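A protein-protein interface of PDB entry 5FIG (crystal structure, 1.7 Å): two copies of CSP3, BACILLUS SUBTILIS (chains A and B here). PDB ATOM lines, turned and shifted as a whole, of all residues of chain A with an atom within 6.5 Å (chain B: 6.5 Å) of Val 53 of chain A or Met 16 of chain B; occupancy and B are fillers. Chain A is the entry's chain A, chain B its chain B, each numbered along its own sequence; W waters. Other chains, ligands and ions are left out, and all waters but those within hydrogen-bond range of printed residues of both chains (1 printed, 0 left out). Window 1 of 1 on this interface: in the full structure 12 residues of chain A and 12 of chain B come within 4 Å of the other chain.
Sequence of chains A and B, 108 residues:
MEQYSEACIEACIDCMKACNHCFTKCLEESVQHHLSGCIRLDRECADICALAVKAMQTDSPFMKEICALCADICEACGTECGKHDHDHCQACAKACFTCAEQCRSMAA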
ATOM      1  N   CYS A   8      17.883 -26.017 -22.843  1.00  0.00           N
ATOM      2  CA  CYS A   8      18.312 -24.639 -22.626  1.00  0.00           C
ATOM      3  C   CYS A   8      17.413 -24.018 -21.545  1.00  0.00           C
ATOM      4  O   CYS A   8      17.913 -23.374 -20.620  1.00  0.00           O
ATOM      5  CB  CYS A   8      18.256 -23.841 -23.882  1.00  0.00           C
ATOM      6  SG  CYS A   8      19.000 -22.243 -23.680  1.00  0.00           S
ATOM      7  N   ILE A   9      16.112 -24.263 -21.660  1.00  0.00           N
ATOM      8  CA  ILE A   9      15.168 -23.835 -20.581  1.00  0.00           C
ATOM      9  C   ILE A   9      15.601 -24.329 -19.224  1.00  0.00           C
ATOM     10  O   ILE A   9      15.626 -23.606 -18.252  1.00  0.00           O
ATOM     11  CB  ILE A   9      13.725 -24.245 -20.920  1.00  0.00           C
ATOM     12  CG1 ILE A   9      13.230 -23.389 -22.095  1.00  0.00           C
ATOM     13  CG2 ILE A   9      12.807 -24.067 -19.715  1.00  0.00           C
ATOM     14  CD1 ILE A   9      12.006 -23.967 -22.801  1.00  0.00           C
ATOM     15  N   GLU A  10      15.869 -25.616 -19.128  1.00  0.00           N
ATOM     16  CA  GLU A  10      16.319 -26.192 -17.885  1.00  0.00           C
ATOM     17  C   GLU A  10      17.561 -25.555 -17.356  1.00  0.00           C
ATOM     18  O   GLU A  10      17.685 -25.320 -16.134  1.00  0.00           O
ATOM     19  CB  GLU A  10      16.477 -27.745 -18.055  1.00  0.00           C
ATOM     20  CG  GLU A  10      15.125 -28.397 -18.095  1.00  0.00           C
ATOM     21  CD  GLU A  10      15.151 -29.901 -18.398  1.00  0.00           C
ATOM     22  OE1 GLU A  10      16.243 -30.458 -18.704  1.00  0.00           O
ATOM     23  OE2 GLU A  10      14.080 -30.554 -18.351  1.00  0.00           O
ATOM     24  N   CYS A  12      18.617 -22.481 -18.014  1.00  0.00           N
ATOM     25  CA  CYS A  12      18.222 -21.155 -17.553  1.00  0.00           C
ATOM     26  C   CYS A  12      17.515 -21.181 -16.167  1.00  0.00           C
ATOM     27  O   CYS A  12      17.809 -20.342 -15.303  1.00  0.00           O
ATOM     28  CB  CYS A  12      17.302 -20.477 -18.582  1.00  0.00           C
ATOM     29  SG  CYS A  12      18.161 -19.996 -20.089  1.00  0.00           S
ATOM     30  N   ILE A  13      16.620 -22.103 -15.982  1.00  0.00           N
ATOM     31  CA  ILE A  13      15.916 -22.254 -14.723  1.00  0.00           C
ATOM     32  C   ILE A  13      16.931 -22.567 -13.602  1.00  0.00           C
ATOM     33  O   ILE A  13      16.875 -22.014 -12.523  1.00  0.00           O
ATOM     34  CB  ILE A  13      14.836 -23.358 -14.793  1.00  0.00           C
ATOM     35  CG1 ILE A  13      13.678 -22.870 -15.682  1.00  0.00           C
ATOM     36  CG2 ILE A  13      14.325 -23.764 -13.407  1.00  0.00           C
ATOM     37  CD1 ILE A  13      12.737 -23.923 -16.139  1.00  0.00           C
ATOM     38  N   MET A  16      18.923 -19.358 -12.889  1.00  0.00           N
ATOM     39  CA  MET A  16      18.092 -18.467 -12.034  1.00  0.00           C
ATOM     40  C   MET A  16      18.155 -18.874 -10.596  1.00  0.00           C
ATOM     41  O   MET A  16      18.284 -18.036  -9.704  1.00  0.00           O
ATOM     42  CB  MET A  16      16.667 -18.492 -12.519  1.00  0.00           C
ATOM     43  CG  MET A  16      15.728 -17.401 -12.188  1.00  0.00           C
ATOM     44  SD  MET A  16      14.127 -17.987 -12.826  1.00  0.00           S
ATOM     45  CE  MET A  16      14.486 -18.575 -14.513  1.00  0.00           C
ATOM     46  N   ILE A  48      17.487 -11.998 -16.745  1.00  0.00           N
ATOM     47  CA  ILE A  48      17.589 -12.330 -18.164  1.00  0.00           C
ATOM     48  C   ILE A  48      17.295 -13.820 -18.415  1.00  0.00           C
ATOM     49  O   ILE A  48      16.768 -14.144 -19.463  1.00  0.00           O
ATOM     50  CB  ILE A  48      18.953 -11.898 -18.808  1.00  0.00           C
ATOM     51  CG1 ILE A  48      18.935 -11.976 -20.339  1.00  0.00           C
ATOM     52  CG2 ILE A  48      20.100 -12.731 -18.350  1.00  0.00           C
ATOM     53  CD1 ILE A  48      18.029 -10.944 -21.016  1.00  0.00           C
ATOM     54  N   CYS A  49      17.680 -14.662 -17.460  1.00  0.00           N
ATOM     55  CA  CYS A  49      17.354 -16.074 -17.595  1.00  0.00           C
ATOM     56  C   CYS A  49      15.844 -16.298 -17.597  1.00  0.00           C
ATOM     57  O   CYS A  49      15.361 -17.049 -18.457  1.00  0.00           O
ATOM     58  CB  CYS A  49      17.994 -16.887 -16.466  1.00  0.00           C
ATOM     59  SG  CYS A  49      19.742 -17.192 -16.668  1.00  0.00           S
ATOM     60  N   ALA A  50      15.109 -15.575 -16.738  1.00  0.00           N
ATOM     61  CA  ALA A  50      13.655 -15.644 -16.758  1.00  0.00           C
ATOM     62  C   ALA A  50      13.059 -15.177 -18.095  1.00  0.00           C
ATOM     63  O   ALA A  50      12.146 -15.786 -18.673  1.00  0.00           O
ATOM     64  CB  ALA A  50      13.094 -14.836 -15.627  1.00  0.00           C
ATOM     65  N   LEU A  51      13.609 -14.097 -18.654  1.00  0.00           N
ATOM     66  CA  LEU A  51      13.187 -13.626 -19.965  1.00  0.00           C
ATOM     67  C   LEU A  51      13.465 -14.618 -21.098  1.00  0.00           C
ATOM     68  O   LEU A  51      12.646 -14.782 -22.047  1.00  0.00           O
ATOM     69  CB  LEU A  51      13.872 -12.290 -20.305  1.00  0.00           C
ATOM     70  CG  LEU A  51      13.444 -11.636 -21.647  1.00  0.00           C
ATOM     71  CD1 LEU A  51      12.066 -11.085 -21.522  1.00  0.00           C
ATOM     72  CD2 LEU A  51      14.403 -10.502 -22.039  1.00  0.00           C
ATOM     73  N   ALA A  52      14.664 -15.224 -21.072  1.00  0.00           N
ATOM     74  CA  ALA A  52      15.000 -16.235 -22.083  1.00  0.00           C
ATOM     75  C   ALA A  52      14.040 -17.444 -22.016  1.00  0.00           C
ATOM     76  O   ALA A  52      13.570 -17.919 -23.058  1.00  0.00           O
ATOM     77  CB  ALA A  52      16.448 -16.671 -21.936  1.00  0.00           C
ATOM     78  N   VAL A  53      13.725 -17.898 -20.800  1.00  0.00           N
ATOM     79  CA  VAL A  53      12.731 -18.950 -20.628  1.00  0.00           C
ATOM     80  C   VAL A  53      11.396 -18.578 -21.279  1.00  0.00           C
ATOM     81  O   VAL A  53      10.816 -19.340 -22.062  1.00  0.00           O
ATOM     82  CB  VAL A  53      12.540 -19.336 -19.188  1.00  0.00           C
ATOM     83  CG1 VAL A  53      11.357 -20.282 -19.015  1.00  0.00           C
ATOM     84  CG2 VAL A  53      13.848 -19.958 -18.673  1.00  0.00           C
ATOM     85  N   LYS A  54      10.925 -17.375 -20.984  1.00  0.00           N
ATOM     86  CA  LYS A  54       9.678 -16.934 -21.575  1.00  0.00           C
ATOM     87  C   LYS A  54       9.749 -16.872 -23.099  1.00  0.00           C
ATOM     88  O   LYS A  54       8.812 -17.290 -23.769  1.00  0.00           O
ATOM     89  CB  LYS A  54       9.321 -15.567 -21.010  1.00  0.00           C
ATOM     90  CG  LYS A  54       7.992 -15.051 -21.454  1.00  0.00           C
ATOM     91  CD  LYS A  54       7.742 -13.588 -21.115  1.00  0.00           C
ATOM     92  CE  LYS A  54       8.325 -13.121 -19.785  1.00  0.00           C
ATOM     93  NZ  LYS A  54       7.750 -11.793 -19.448  1.00  0.00           N
ATOM     94  N   ALA A  55      10.851 -16.350 -23.624  1.00  0.00           N
ATOM     95  CA  ALA A  55      11.049 -16.263 -25.065  1.00  0.00           C
ATOM     96  C   ALA A  55      11.025 -17.614 -25.737  1.00  0.00           C
ATOM     97  O   ALA A  55      10.336 -17.811 -26.752  1.00  0.00           O
ATOM     98  CB  ALA A  55      12.351 -15.559 -25.389  1.00  0.00           C
ATOM     99  N   MET A  56      11.714 -18.570 -25.134  1.00  0.00           N
ATOM    100  CA  MET A  56      11.687 -19.940 -25.685  1.00  0.00           C
ATOM    101  C   MET A  56      10.321 -20.592 -25.570  1.00  0.00           C
ATOM    102  O   MET A  56       9.866 -21.266 -26.511  1.00  0.00           O
ATOM    103  CB  MET A  56      12.757 -20.796 -25.038  1.00  0.00           C
ATOM    104  CG  MET A  56      14.147 -20.365 -25.418  1.00  0.00           C
ATOM    105  SD  MET A  56      15.452 -21.410 -24.663  1.00  0.00           S
ATOM    106  CE  MET A  56      15.708 -20.644 -23.089  1.00  0.00           C
ATOM    107  N   GLN A  57       9.655 -20.413 -24.451  1.00  0.00           N
ATOM    108  CA  GLN A  57       8.354 -21.078 -24.244  1.00  0.00           C
ATOM    109  C   GLN A  57       7.265 -20.506 -25.132  1.00  0.00           C
ATOM    110  O   GLN A  57       6.292 -21.180 -25.438  1.00  0.00           O
ATOM    111  CB  GLN A  57       7.930 -21.009 -22.786  1.00  0.00           C
ATOM    112  CG  GLN A  57       8.805 -21.834 -21.895  1.00  0.00           C
ATOM    113  CD  GLN A  57       8.442 -21.760 -20.410  1.00  0.00           C
ATOM    114  OE1 GLN A  57       7.829 -20.812 -19.943  1.00  0.00           O
ATOM    115  NE2 GLN A  57       8.841 -22.786 -19.675  1.00  0.00           N
ATOM    116  N   THR A  58       7.392 -19.226 -25.488  1.00  0.00           N
ATOM    117  CA  THR A  58       6.406 -18.556 -26.287  1.00  0.00           C
ATOM    118  C   THR A  58       6.787 -18.483 -27.769  1.00  0.00           C
ATOM    119  O   THR A  58       6.016 -17.922 -28.542  1.00  0.00           O
ATOM    120  CB  THR A  58       6.123 -17.085 -25.822  1.00  0.00           C
ATOM    121  OG1 THR A  58       7.316 -16.319 -25.930  1.00  0.00           O
ATOM    122  CG2 THR A  58       5.561 -17.054 -24.362  1.00  0.00           C
ATOM    123  N   ILE A  66      17.629 -13.051 -27.758  1.00  0.00           N
ATOM    124  CA  ILE A  66      17.503 -13.024 -26.303  1.00  0.00           C
ATOM    125  C   ILE A  66      18.444 -14.078 -25.690  1.00  0.00           C
ATOM    126  O   ILE A  66      19.144 -13.791 -24.695  1.00  0.00           O
ATOM    127  CB  ILE A  66      16.040 -13.163 -25.850  1.00  0.00           C
ATOM    128  CG1 ILE A  66      15.263 -11.902 -26.258  1.00  0.00           C
ATOM    129  CG2 ILE A  66      15.941 -13.463 -24.351  1.00  0.00           C
ATOM    130  CD1 ILE A  66      13.756 -12.049 -26.168  1.00  0.00           C
ATOM    131  N   ALA B  11       5.633 -25.826  -8.935  1.00  0.00           N
ATOM    132  CA  ALA B  11       4.289 -25.548  -9.472  1.00  0.00           C
ATOM    133  C   ALA B  11       4.206 -24.260 -10.264  1.00  0.00           C
ATOM    134  O   ALA B  11       3.548 -24.212 -11.307  1.00  0.00           O
ATOM    135  CB  ALA B  11       3.272 -25.545  -8.378  1.00  0.00           C
ATOM    136  N   CYS B  12       4.901 -23.221  -9.803  1.00  0.00           N
ATOM    137  CA  CYS B  12       4.965 -21.959 -10.543  1.00  0.00           C
ATOM    138  C   CYS B  12       5.699 -22.136 -11.881  1.00  0.00           C
ATOM    139  O   CYS B  12       5.256 -21.616 -12.937  1.00  0.00           O
ATOM    140  CB  CYS B  12       5.678 -20.864  -9.737  1.00  0.00           C
ATOM    141  SG  CYS B  12       4.720 -20.255  -8.345  1.00  0.00           S
ATOM    142  N   ILE B  13       6.791 -22.866 -11.854  1.00  0.00           N
ATOM    143  CA  ILE B  13       7.570 -23.124 -13.106  1.00  0.00           C
ATOM    144  C   ILE B  13       6.666 -23.892 -14.106  1.00  0.00           C
ATOM    145  O   ILE B  13       6.636 -23.626 -15.286  1.00  0.00           O
ATOM    146  CB  ILE B  13       8.875 -23.869 -12.786  1.00  0.00           C
ATOM    147  CG1 ILE B  13       9.833 -22.922 -12.043  1.00  0.00           C
ATOM    148  CG2 ILE B  13       9.501 -24.443 -14.047  1.00  0.00           C
ATOM    149  CD1 ILE B  13      10.979 -23.609 -11.377  1.00  0.00           C
ATOM    150  N   ASP B  14       5.951 -24.931 -13.600  1.00  0.00           N
ATOM    151  CA  ASP B  14       5.049 -25.691 -14.450  1.00  0.00           C
ATOM    152  C   ASP B  14       3.915 -24.859 -15.017  1.00  0.00           C
ATOM    153  O   ASP B  14       3.433 -25.089 -16.130  1.00  0.00           O
ATOM    154  CB  ASP B  14       4.487 -26.927 -13.672  1.00  0.00           C
ATOM    155  CG  ASP B  14       5.531 -27.991 -13.381  1.00  0.00           C
ATOM    156  OD1 ASP B  14       6.616 -27.972 -13.944  1.00  0.00           O
ATOM    157  OD2 ASP B  14       5.315 -28.892 -12.555  1.00  0.00           O
ATOM    158  N   CYS B  15       3.410 -23.932 -14.205  1.00  0.00           N
ATOM    159  CA  CYS B  15       2.324 -23.087 -14.623  1.00  0.00           C
ATOM    160  C   CYS B  15       2.815 -22.119 -15.733  1.00  0.00           C
ATOM    161  O   CYS B  15       2.118 -21.869 -16.697  1.00  0.00           O
ATOM    162  CB  CYS B  15       1.746 -22.374 -13.429  1.00  0.00           C
ATOM    163  SG  CYS B  15       0.288 -21.407 -13.817  1.00  0.00           S
ATOM    164  N   MET B  16       3.984 -21.540 -15.532  1.00  0.00           N
ATOM    165  CA  MET B  16       4.619 -20.682 -16.555  1.00  0.00           C
ATOM    166  C   MET B  16       4.717 -21.398 -17.860  1.00  0.00           C
ATOM    167  O   MET B  16       4.389 -20.853 -18.898  1.00  0.00           O
ATOM    168  CB  MET B  16       5.988 -20.263 -16.104  1.00  0.00           C
ATOM    169  CG  MET B  16       6.661 -19.099 -16.725  1.00  0.00           C
ATOM    170  SD  MET B  16       8.315 -19.118 -16.013  1.00  0.00           S
ATOM    171  CE  MET B  16       9.104 -18.155 -17.273  1.00  0.00           C
ATOM    172  N   LYS B  17       5.232 -22.626 -17.809  1.00  0.00           N
ATOM    173  CA  LYS B  17       5.355 -23.407 -19.005  1.00  0.00           C
ATOM    174  C   LYS B  17       3.995 -23.541 -19.686  1.00  0.00           C
ATOM    175  O   LYS B  17       3.858 -23.390 -20.871  1.00  0.00           O
ATOM    176  CB  LYS B  17       5.932 -24.787 -18.662  1.00  0.00           C
ATOM    177  CG  LYS B  17       6.077 -25.713 -19.834  1.00  0.00           C
ATOM    178  CD  LYS B  17       6.695 -27.040 -19.409  1.00  0.00           C
ATOM    179  CE  LYS B  17       6.815 -27.935 -20.624  1.00  0.00           C
ATOM    180  NZ  LYS B  17       7.262 -29.325 -20.320  1.00  0.00           N
ATOM    181  N   ALA B  18       3.005 -23.972 -18.921  1.00  0.00           N
ATOM    182  CA  ALA B  18       1.683 -24.233 -19.508  1.00  0.00           C
ATOM    183  C   ALA B  18       1.018 -22.992 -20.079  1.00  0.00           C
ATOM    184  O   ALA B  18       0.433 -23.023 -21.152  1.00  0.00           O
ATOM    185  CB  ALA B  18       0.766 -24.895 -18.457  1.00  0.00           C
ATOM    186  N   CYS B  19       1.126 -21.891 -19.348  1.00  0.00           N
ATOM    187  CA  CYS B  19       0.580 -20.589 -19.774  1.00  0.00           C
ATOM    188  C   CYS B  19       1.273 -20.076 -20.988  1.00  0.00           C
ATOM    189  O   CYS B  19       0.611 -19.622 -21.949  1.00  0.00           O
ATOM    190  CB  CYS B  19       0.704 -19.520 -18.630  1.00  0.00           C
ATOM    191  SG  CYS B  19      -0.510 -19.799 -17.304  1.00  0.00           S
ATOM    192  N   ASN B  20       2.609 -20.171 -21.012  1.00  0.00           N
ATOM    193  CA  ASN B  20       3.343 -19.736 -22.227  1.00  0.00           C
ATOM    194  C   ASN B  20       3.026 -20.598 -23.464  1.00  0.00           C
ATOM    195  O   ASN B  20       2.906 -20.110 -24.570  1.00  0.00           O
ATOM    196  CB  ASN B  20       4.854 -19.703 -21.966  1.00  0.00           C
ATOM    197  CG  ASN B  20       5.281 -18.527 -21.129  1.00  0.00           C
ATOM    198  OD1 ASN B  20       4.666 -17.495 -21.215  1.00  0.00           O
ATOM    199  ND2 ASN B  20       6.335 -18.677 -20.310  1.00  0.00           N
ATOM    200  N   HIS B  21       2.927 -21.918 -23.260  1.00  0.00           N
ATOM    201  CA  HIS B  21       2.497 -22.793 -24.319  1.00  0.00           C
ATOM    202  C   HIS B  21       1.093 -22.487 -24.833  1.00  0.00           C
ATOM    203  O   HIS B  21       0.858 -22.499 -26.046  1.00  0.00           O
ATOM    204  CB  HIS B  21       2.608 -24.279 -23.870  1.00  0.00           C
ATOM    205  CG  HIS B  21       4.034 -24.752 -23.847  1.00  0.00           C
ATOM    206  ND1 HIS B  21       4.390 -25.945 -23.253  1.00  0.00           N
ATOM    207  CD2 HIS B  21       5.206 -24.190 -24.273  1.00  0.00           C
ATOM    208  CE1 HIS B  21       5.694 -26.133 -23.354  1.00  0.00           C
ATOM    209  NE2 HIS B  21       6.216 -25.090 -23.975  1.00  0.00           N
ATOM    210  N   ASP B  42      -3.006 -15.535 -19.863  1.00  0.00           N
ATOM    211  CA  ASP B  42      -1.796 -16.397 -19.991  1.00  0.00           C
ATOM    212  C   ASP B  42      -0.535 -15.555 -19.835  1.00  0.00           C
ATOM    213  O   ASP B  42       0.439 -15.984 -19.191  1.00  0.00           O
ATOM    214  CB  ASP B  42      -1.708 -17.067 -21.360  1.00  0.00           C
ATOM    215  CG  ASP B  42      -2.628 -18.259 -21.507  1.00  0.00           C
ATOM    216  OD1 ASP B  42      -2.998 -18.886 -20.489  1.00  0.00           O
ATOM    217  OD2 ASP B  42      -2.967 -18.567 -22.686  1.00  0.00           O
ATOM    218  N   CYS B  45      -0.337 -14.365 -16.118  1.00  0.00           N
ATOM    219  CA  CYS B  45      -0.101 -15.461 -15.171  1.00  0.00           C
ATOM    220  C   CYS B  45       1.337 -15.985 -15.291  1.00  0.00           C
ATOM    221  O   CYS B  45       2.039 -16.102 -14.284  1.00  0.00           O
ATOM    222  CB  CYS B  45      -1.094 -16.557 -15.443  1.00  0.00           C
ATOM    223  SG  CYS B  45      -0.993 -17.882 -14.231  1.00  0.00           S
ATOM    224  N   ALA B  46       1.806 -16.130 -16.515  1.00  0.00           N
ATOM    225  CA  ALA B  46       3.235 -16.516 -16.723  1.00  0.00           C
ATOM    226  C   ALA B  46       4.191 -15.506 -16.092  1.00  0.00           C
ATOM    227  O   ALA B  46       5.192 -15.861 -15.425  1.00  0.00           O
ATOM    228  CB  ALA B  46       3.552 -16.630 -18.179  1.00  0.00           C
ATOM    229  N   ASP B  47       3.873 -14.226 -16.250  1.00  0.00           N
ATOM    230  CA  ASP B  47       4.717 -13.174 -15.677  1.00  0.00           C
ATOM    231  C   ASP B  47       4.742 -13.185 -14.150  1.00  0.00           C
ATOM    232  O   ASP B  47       5.805 -13.033 -13.511  1.00  0.00           O
ATOM    233  CB  ASP B  47       4.318 -11.776 -16.215  1.00  0.00           C
ATOM    234  CG  ASP B  47       4.585 -11.593 -17.724  1.00  0.00           C
ATOM    235  OD1 ASP B  47       5.228 -12.438 -18.412  1.00  0.00           O
ATOM    236  OD2 ASP B  47       4.211 -10.512 -18.235  1.00  0.00           O
ATOM    237  N   CYS B  49       3.999 -15.687 -12.189  1.00  0.00           N
ATOM    238  CA  CYS B  49       4.614 -16.915 -11.718  1.00  0.00           C
ATOM    239  C   CYS B  49       6.145 -16.774 -11.684  1.00  0.00           C
ATOM    240  O   CYS B  49       6.769 -17.192 -10.695  1.00  0.00           O
ATOM    241  CB  CYS B  49       4.255 -18.139 -12.602  1.00  0.00           C
ATOM    242  SG  CYS B  49       2.590 -18.776 -12.299  1.00  0.00           S
ATOM    243  N   ALA B  50       6.710 -16.155 -12.717  1.00  0.00           N
ATOM    244  CA  ALA B  50       8.139 -15.887 -12.735  1.00  0.00           C
ATOM    245  C   ALA B  50       8.525 -14.997 -11.526  1.00  0.00           C
ATOM    246  O   ALA B  50       9.567 -15.189 -10.873  1.00  0.00           O
ATOM    247  CB  ALA B  50       8.521 -15.229 -14.029  1.00  0.00           C
ATOM    248  N   VAL B  53       8.497 -17.013  -8.272  1.00  0.00           N
ATOM    249  CA  VAL B  53       9.732 -17.839  -8.209  1.00  0.00           C
ATOM    250  C   VAL B  53      10.907 -17.005  -7.712  1.00  0.00           C
ATOM    251  O   VAL B  53      11.625 -17.396  -6.795  1.00  0.00           O
ATOM    252  CB  VAL B  53      10.029 -18.506  -9.533  1.00  0.00           C
ATOM    253  CG1 VAL B  53      11.408 -19.154  -9.515  1.00  0.00           C
ATOM    254  CG2 VAL B  53       8.934 -19.550  -9.833  1.00  0.00           C
ATOM    255  N   ALA B  95      -2.789 -26.740 -14.477  1.00  0.00           N
ATOM    256  CA  ALA B  95      -1.530 -26.230 -13.908  1.00  0.00           C
ATOM    257  C   ALA B  95      -1.781 -24.961 -13.125  1.00  0.00           C
ATOM    258  O   ALA B  95      -1.147 -24.744 -12.110  1.00  0.00           O
ATOM    259  CB  ALA B  95      -0.489 -26.002 -14.995  1.00  0.00           C
HETATM  260  O   HOH W   1       8.794 -22.700 -16.848  1.00  0.00           O
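OD1 of Asp 47 of chain B is in salt-bridge range of NZ of Lys 54 of chain A. The side-chain amide oxygen (OE1) of Gln 57 of chain A sits at hydrogen-bond distance from the side-chain amide nitrogen (ND2) of Asn 20 of chain B (2.6 Å).
The backbone carbonyl oxygen (O) of Lys 54 of chain A lies within hydrogen-bond range of the side-chain hydroxyl (OG1) of Thr 58 of chain A. O of Ala 55 of chain A lies within hydrogen-bond range of OG1 of Thr 58 of chain A (3.5 Å). The backbone carbonyl oxygen of Met 16 of chain B sits at hydrogen-bond distance from the side-chain amide nitrogen of Asn 20 of chain B (3.2 Å).
Ile 13 of chain A touches Ile 13 of chain B (CD1 to CG2, 3.9 Å). CE of Met 16 of chain B touches CG1 of Val 53 of chain A, 3.6 Å away. CA of Lys 54 of chain A touches ND2 of Asn 20 of chain B, 3.98 Å away. Met 16 of chain B touches Gln 57 of chain A (O to OE1, 3.6 Å). Lys 17 of chain B touches Gln 57 of chain A. His 21 of chain B touches Gln 57 of chain A (CD2 to O, 3.4 Å). Asn 20 of chain B touches Thr 58 of chain A.
Printed residues of chain B within 4 Å of Ile 13 of chain A: Ile 13 (3.9 Å). Of the printed residues of chain B, Val 53 of chain A touches Met 16. Printed residues of chain B within 4 Å of Lys 54 of chain A: Asn 20 and Asp 47. Of the printed residues of chain A, Met 16 of chain B touches Val 53 (3.6 Å) and Gln 57 (3.6 Å). Of the printed residues of chain A, His 21 of chain B touches Gln 57 (3.4 Å). The nearest printed residue of chain A that does not touch His 21 of chain B is Thr 58 of chain A (5.6 Å).
Of the 19 printed residues of chain B, 6 touch a printed residue of chain A. Printed residues of chain B that touch a printed residue of chain A: Ile 13, Met 16, Lys 17, Asn 20, His 21 and Asp 47. Hydrophobic or aromatic side chains of chain B within 4 Å of the printed part of chain A: Ile 13, Met 16 and His 21. Hydrophobic or aromatic side chains of chain A that line the printed part of chain B: Ile 13 and Val 53.
Ile 13 of chain A touches its own counterpart, Ile 13 of chain B. Val 53 of chain A touches Met 16 of chain B, but with the chains exchanged Met 16 of chain A does not touch Val 53 of chain B (4.4 Å).
Water W1 lies within hydrogen-bond range of O of Ile 13 of chain B, NE2 of Gln 57 of chain A and SD of Met 16 of chain B.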
